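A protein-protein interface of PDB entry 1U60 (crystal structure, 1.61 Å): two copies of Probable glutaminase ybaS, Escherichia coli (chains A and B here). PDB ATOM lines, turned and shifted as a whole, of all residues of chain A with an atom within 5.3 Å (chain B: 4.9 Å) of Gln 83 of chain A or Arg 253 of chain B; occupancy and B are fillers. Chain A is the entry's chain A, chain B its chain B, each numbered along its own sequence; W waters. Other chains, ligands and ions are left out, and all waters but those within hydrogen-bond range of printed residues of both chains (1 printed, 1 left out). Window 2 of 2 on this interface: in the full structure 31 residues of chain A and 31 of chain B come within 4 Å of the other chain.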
ATOM      1  N   GLY A  81       7.394 -29.962 -11.149  1.00  0.00           N
ATOM      2  CA  GLY A  81       8.531 -29.587 -11.979  1.00  0.00           C
ATOM      3  C   GLY A  81       8.174 -29.532 -13.455  1.00  0.00           C
ATOM      4  O   GLY A  81       7.102 -30.016 -13.840  1.00  0.00           O
ATOM      5  N   PRO A  82       9.045 -28.965 -14.277  1.00  0.00           N
ATOM      6  CA  PRO A  82       8.704 -28.741 -15.685  1.00  0.00           C
ATOM      7  C   PRO A  82       8.554 -29.970 -16.536  1.00  0.00           C
ATOM      8  O   PRO A  82       7.716 -29.968 -17.464  1.00  0.00           O
ATOM      9  CB  PRO A  82       9.850 -27.846 -16.207  1.00  0.00           C
ATOM     10  CG  PRO A  82      10.980 -28.100 -15.209  1.00  0.00           C
ATOM     11  CD  PRO A  82      10.325 -28.305 -13.929  1.00  0.00           C
ATOM     12  N   GLN A  83       9.338 -31.020 -16.264  1.00  0.00           N
ATOM     13  CA  GLN A  83       9.191 -32.227 -17.077  1.00  0.00           C
ATOM     14  C   GLN A  83       7.804 -32.838 -16.912  1.00  0.00           C
ATOM     15  O   GLN A  83       7.158 -33.203 -17.885  1.00  0.00           O
ATOM     16  CB  GLN A  83      10.296 -33.287 -16.793  1.00  0.00           C
ATOM     17  CG  GLN A  83      10.216 -34.442 -17.789  1.00  0.00           C
ATOM     18  CD  GLN A  83      10.532 -33.990 -19.206  1.00  0.00           C
ATOM     19  OE1 GLN A  83      11.599 -33.444 -19.453  1.00  0.00           O
ATOM     20  NE2 GLN A  83       9.590 -34.165 -20.116  1.00  0.00           N
ATOM     21  N   ALA A  84       7.314 -32.923 -15.672  1.00  0.00           N
ATOM     22  CA  ALA A  84       6.010 -33.441 -15.412  1.00  0.00           C
ATOM     23  C   ALA A  84       4.912 -32.621 -16.036  1.00  0.00           C
ATOM     24  O   ALA A  84       3.930 -33.178 -16.501  1.00  0.00           O
ATOM     25  CB  ALA A  84       5.801 -33.564 -13.877  1.00  0.00           C
ATOM     26  N   VAL A  85       5.022 -31.291 -15.984  1.00  0.00           N
ATOM     27  CA  VAL A  85       4.041 -30.464 -16.604  1.00  0.00           C
ATOM     28  C   VAL A  85       4.026 -30.693 -18.125  1.00  0.00           C
ATOM     29  O   VAL A  85       2.973 -30.804 -18.726  1.00  0.00           O
ATOM     30  CB  VAL A  85       4.250 -28.980 -16.241  1.00  0.00           C
ATOM     31  CG1 VAL A  85       3.368 -28.074 -17.118  1.00  0.00           C
ATOM     32  CG2 VAL A  85       3.915 -28.765 -14.758  1.00  0.00           C
ATOM     33  N   GLN A  86       5.188 -30.837 -18.727  1.00  0.00           N
ATOM     34  CA  GLN A  86       5.271 -31.029 -20.200  1.00  0.00           C
ATOM     35  C   GLN A  86       4.663 -32.405 -20.608  1.00  0.00           C
ATOM     36  O   GLN A  86       3.944 -32.512 -21.621  1.00  0.00           O
ATOM     37  CB  GLN A  86       6.718 -30.905 -20.667  1.00  0.00           C
ATOM     38  CG  GLN A  86       6.804 -30.793 -22.174  1.00  0.00           C
ATOM     39  CD  GLN A  86       8.234 -30.623 -22.668  1.00  0.00           C
ATOM     40  OE1 GLN A  86       9.192 -30.743 -21.886  1.00  0.00           O
ATOM     41  NE2 GLN A  86       8.376 -30.262 -23.959  1.00  0.00           N
ATOM     42  N   ASP A  87       4.932 -33.437 -19.813  1.00  0.00           N
ATOM     43  CA  ASP A  87       4.442 -34.782 -20.053  1.00  0.00           C
ATOM     44  C   ASP A  87       2.931 -34.928 -19.803  1.00  0.00           C
ATOM     45  O   ASP A  87       2.205 -35.573 -20.591  1.00  0.00           O
ATOM     46  CB  ASP A  87       5.146 -35.754 -19.098  1.00  0.00           C
ATOM     47  CG  ASP A  87       6.616 -35.989 -19.448  1.00  0.00           C
ATOM     48  OD1 ASP A  87       7.070 -35.653 -20.569  1.00  0.00           O
ATOM     49  OD2 ASP A  87       7.388 -36.509 -18.627  1.00  0.00           O
ATOM     50  N   LYS A  88       2.459 -34.362 -18.690  1.00  0.00           N
ATOM     51  CA  LYS A  88       1.081 -34.553 -18.235  1.00  0.00           C
ATOM     52  C   LYS A  88       0.074 -33.518 -18.761  1.00  0.00           C
ATOM     53  O   LYS A  88      -1.119 -33.780 -18.757  1.00  0.00           O
ATOM     54  CB  LYS A  88       1.060 -34.581 -16.701  1.00  0.00           C
ATOM     55  CG  LYS A  88       2.007 -35.621 -16.097  1.00  0.00           C
ATOM     56  CD  LYS A  88       1.622 -37.024 -16.525  1.00  0.00           C
ATOM     57  CE  LYS A  88       2.414 -38.080 -15.704  1.00  0.00           C
ATOM     58  NZ  LYS A  88       2.233 -39.504 -16.222  1.00  0.00           N
ATOM     59  N   TYR A 233       9.387 -21.198 -18.195  1.00  0.00           N
ATOM     60  CA  TYR A 233       8.407 -22.168 -18.683  1.00  0.00           C
ATOM     61  C   TYR A 233       7.028 -21.528 -18.703  1.00  0.00           C
ATOM     62  O   TYR A 233       6.226 -21.756 -19.596  1.00  0.00           O
ATOM     63  CB  TYR A 233       8.367 -23.378 -17.765  1.00  0.00           C
ATOM     64  CG  TYR A 233       9.674 -24.155 -17.736  1.00  0.00           C
ATOM     65  CD1 TYR A 233      10.088 -24.910 -18.842  1.00  0.00           C
ATOM     66  CD2 TYR A 233      10.482 -24.141 -16.600  1.00  0.00           C
ATOM     67  CE1 TYR A 233      11.268 -25.601 -18.810  1.00  0.00           C
ATOM     68  CE2 TYR A 233      11.649 -24.847 -16.558  1.00  0.00           C
ATOM     69  CZ  TYR A 233      12.054 -25.560 -17.670  1.00  0.00           C
ATOM     70  OH  TYR A 233      13.211 -26.278 -17.614  1.00  0.00           O
ATOM     71  N   ASP B 249       7.079 -26.873 -27.485  1.00  0.00           N
ATOM     72  CA  ASP B 249       8.097 -27.599 -26.734  1.00  0.00           C
ATOM     73  C   ASP B 249       9.452 -26.943 -26.836  1.00  0.00           C
ATOM     74  O   ASP B 249      10.186 -26.915 -25.864  1.00  0.00           O
ATOM     75  CB  ASP B 249       8.184 -29.040 -27.198  1.00  0.00           C
ATOM     76  CG  ASP B 249       6.879 -29.725 -27.117  1.00  0.00           C
ATOM     77  OD1 ASP B 249       6.364 -29.872 -25.984  1.00  0.00           O
ATOM     78  OD2 ASP B 249       6.273 -30.126 -28.144  1.00  0.00           O
ATOM     79  N   TRP B 250       9.809 -26.483 -28.046  1.00  0.00           N
ATOM     80  CA  TRP B 250      11.011 -25.732 -28.244  1.00  0.00           C
ATOM     81  C   TRP B 250      11.032 -24.426 -27.438  1.00  0.00           C
ATOM     82  O   TRP B 250      12.014 -24.118 -26.790  1.00  0.00           O
ATOM     83  CB  TRP B 250      11.247 -25.510 -29.721  1.00  0.00           C
ATOM     84  CG  TRP B 250      12.535 -24.818 -30.055  1.00  0.00           C
ATOM     85  CD1 TRP B 250      12.744 -23.506 -30.248  1.00  0.00           C
ATOM     86  CD2 TRP B 250      13.839 -25.456 -30.178  1.00  0.00           C
ATOM     87  NE1 TRP B 250      14.079 -23.275 -30.516  1.00  0.00           N
ATOM     88  CE2 TRP B 250      14.765 -24.457 -30.478  1.00  0.00           C
ATOM     89  CE3 TRP B 250      14.289 -26.774 -30.090  1.00  0.00           C
ATOM     90  CZ2 TRP B 250      16.116 -24.729 -30.689  1.00  0.00           C
ATOM     91  CZ3 TRP B 250      15.634 -27.033 -30.291  1.00  0.00           C
ATOM     92  CH2 TRP B 250      16.510 -26.034 -30.569  1.00  0.00           C
ATOM     93  N   ALA B 251       9.927 -23.685 -27.456  1.00  0.00           N
ATOM     94  CA  ALA B 251       9.841 -22.439 -26.690  1.00  0.00           C
ATOM     95  C   ALA B 251       9.995 -22.736 -25.169  1.00  0.00           C
ATOM     96  O   ALA B 251      10.685 -22.034 -24.434  1.00  0.00           O
ATOM     97  CB  ALA B 251       8.517 -21.802 -26.955  1.00  0.00           C
ATOM     98  N   TYR B 252       9.418 -23.839 -24.738  1.00  0.00           N
ATOM     99  CA  TYR B 252       9.426 -24.238 -23.346  1.00  0.00           C
ATOM    100  C   TYR B 252      10.813 -24.655 -22.860  1.00  0.00           C
ATOM    101  O   TYR B 252      11.240 -24.273 -21.758  1.00  0.00           O
ATOM    102  CB  TYR B 252       8.451 -25.417 -23.249  1.00  0.00           C
ATOM    103  CG  TYR B 252       8.081 -25.955 -21.882  1.00  0.00           C
ATOM    104  CD1 TYR B 252       7.076 -25.365 -21.134  1.00  0.00           C
ATOM    105  CD2 TYR B 252       8.691 -27.107 -21.385  1.00  0.00           C
ATOM    106  CE1 TYR B 252       6.693 -25.851 -19.930  1.00  0.00           C
ATOM    107  CE2 TYR B 252       8.300 -27.624 -20.144  1.00  0.00           C
ATOM    108  CZ  TYR B 252       7.299 -26.998 -19.436  1.00  0.00           C
ATOM    109  OH  TYR B 252       6.839 -27.484 -18.218  1.00  0.00           O
ATOM    110  N   ARG B 253      11.506 -25.467 -23.664  1.00  0.00           N
ATOM    111  CA  ARG B 253      12.815 -25.974 -23.269  1.00  0.00           C
ATOM    112  C   ARG B 253      13.986 -25.052 -23.576  1.00  0.00           C
ATOM    113  O   ARG B 253      14.928 -24.968 -22.787  1.00  0.00           O
ATOM    114  CB  ARG B 253      13.060 -27.343 -23.897  1.00  0.00           C
ATOM    115  CG  ARG B 253      12.079 -28.412 -23.370  1.00  0.00           C
ATOM    116  CD  ARG B 253      12.267 -28.828 -21.916  1.00  0.00           C
ATOM    117  NE  ARG B 253      13.304 -29.852 -21.738  1.00  0.00           N
ATOM    118  CZ  ARG B 253      13.218 -31.130 -22.127  1.00  0.00           C
ATOM    119  NH1 ARG B 253      12.130 -31.615 -22.725  1.00  0.00           N
ATOM    120  NH2 ARG B 253      14.245 -31.931 -21.900  1.00  0.00           N
ATOM    121  N   VAL B 254      13.955 -24.415 -24.749  1.00  0.00           N
ATOM    122  CA  VAL B 254      15.046 -23.591 -25.260  1.00  0.00           C
ATOM    123  C   VAL B 254      14.791 -22.070 -25.178  1.00  0.00           C
ATOM    124  O   VAL B 254      15.678 -21.318 -24.791  1.00  0.00           O
ATOM    125  CB  VAL B 254      15.373 -23.984 -26.726  1.00  0.00           C
ATOM    126  CG1 VAL B 254      16.540 -23.182 -27.224  1.00  0.00           C
ATOM    127  CG2 VAL B 254      15.590 -25.483 -26.855  1.00  0.00           C
ATOM    128  N   GLY B 255      13.568 -21.626 -25.556  1.00  0.00           N
ATOM    129  CA  GLY B 255      13.203 -20.225 -25.444  1.00  0.00           C
ATOM    130  C   GLY B 255      13.889 -19.290 -26.401  1.00  0.00           C
ATOM    131  O   GLY B 255      14.049 -18.123 -26.103  1.00  0.00           O
ATOM    132  N   ASN B 306      17.873 -17.338 -23.524  1.00  0.00           N
ATOM    133  CA  ASN B 306      16.455 -17.694 -23.521  1.00  0.00           C
ATOM    134  C   ASN B 306      15.750 -16.352 -23.445  1.00  0.00           C
ATOM    135  O   ASN B 306      15.958 -15.587 -22.471  1.00  0.00           O
ATOM    136  CB  ASN B 306      16.165 -18.582 -22.287  1.00  0.00           C
ATOM    137  CG  ASN B 306      14.730 -19.055 -22.186  1.00  0.00           C
ATOM    138  OD1 ASN B 306      13.818 -18.296 -22.435  1.00  0.00           O
ATOM    139  ND2 ASN B 306      14.524 -20.290 -21.725  1.00  0.00           N
HETATM  140  O   HOH W   1      14.643 -26.589 -20.291  1.00  0.00           O
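Among the printed residues, pairs that only touch across the chains: Tyr 233 of chain A with Tyr 252 of chain B (3.2 Å), Val 85 of chain A with Tyr 252 of chain B (3.6 Å), Gln 86 of chain A with Tyr 252 of chain B (3.7 Å) and Gln 83 of chain A with Arg 253 of chain B (3.8 Å).
The side-chain amide oxygen (OE1) of Gln 86 of chain A lies within hydrogen-bond range of the guanidinium group (NH1) of Arg 253 of chain B, 3.2 Å away.
NE2 of Gln 86 of chain A is in hydrogen-bond range of OD1 of Asp 249 of chain B (2.9 Å).
The side-chain hydroxyl of Tyr 252 of chain B sits at hydrogen-bond distance from the backbone carbonyl oxygen of Pro 82 of chain A.
Water W1 bridges the backbone carbonyl oxygen of Arg 253 of chain B (3.0 Å) and the side-chain hydroxyl of Tyr 233 of chain A (3.1 Å).
Gln 83 of chain A touches just one residue of chain B: Arg 253.
Printed residues of chain B within 4 Å of Gln 86 of chain A: Asp 249 (2.9 Å), Tyr 252 (3.7 Å) and Arg 253 (3.2 Å).
Printed residues of chain A within 4 Å of Asp 249 of chain B: Gln 86.
Printed residues of chain A within 4 Å of Tyr 252 of chain B: Pro 82, Val 85, Gln 86 and Tyr 233.
Of the printed residues of chain A, Arg 253 of chain B touches Gln 83 (3.8 Å) and Gln 86 (3.2 Å).
Val 254 of chain B touches none of the printed residues of chain A.
Gly 255 of chain B touches none of the printed residues of chain A.
The nearest printed residue of chain B that does not touch Val 85 of chain A is Asp 249 of chain B (8.1 Å).
Hydrophobic or aromatic side chains of chain B that line the printed part of chain A: Tyr 252.
Along chain B the printed residues that touch a printed residue of chain A span positions 249 to 253.
Hydrophobic or aromatic side chains of chain A that line the printed part of chain B: Pro 82, Val 85 and Tyr 233.
NE2 of Gln 83 of chain A sits at hydrogen-bond distance from OD1 of Asp 87 of chain A (3.0 Å).
No position is printed for both chains.
Of the 7 pairs that touch across the chains among the printed residues, none has its exchanged pair printed and touching as well.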
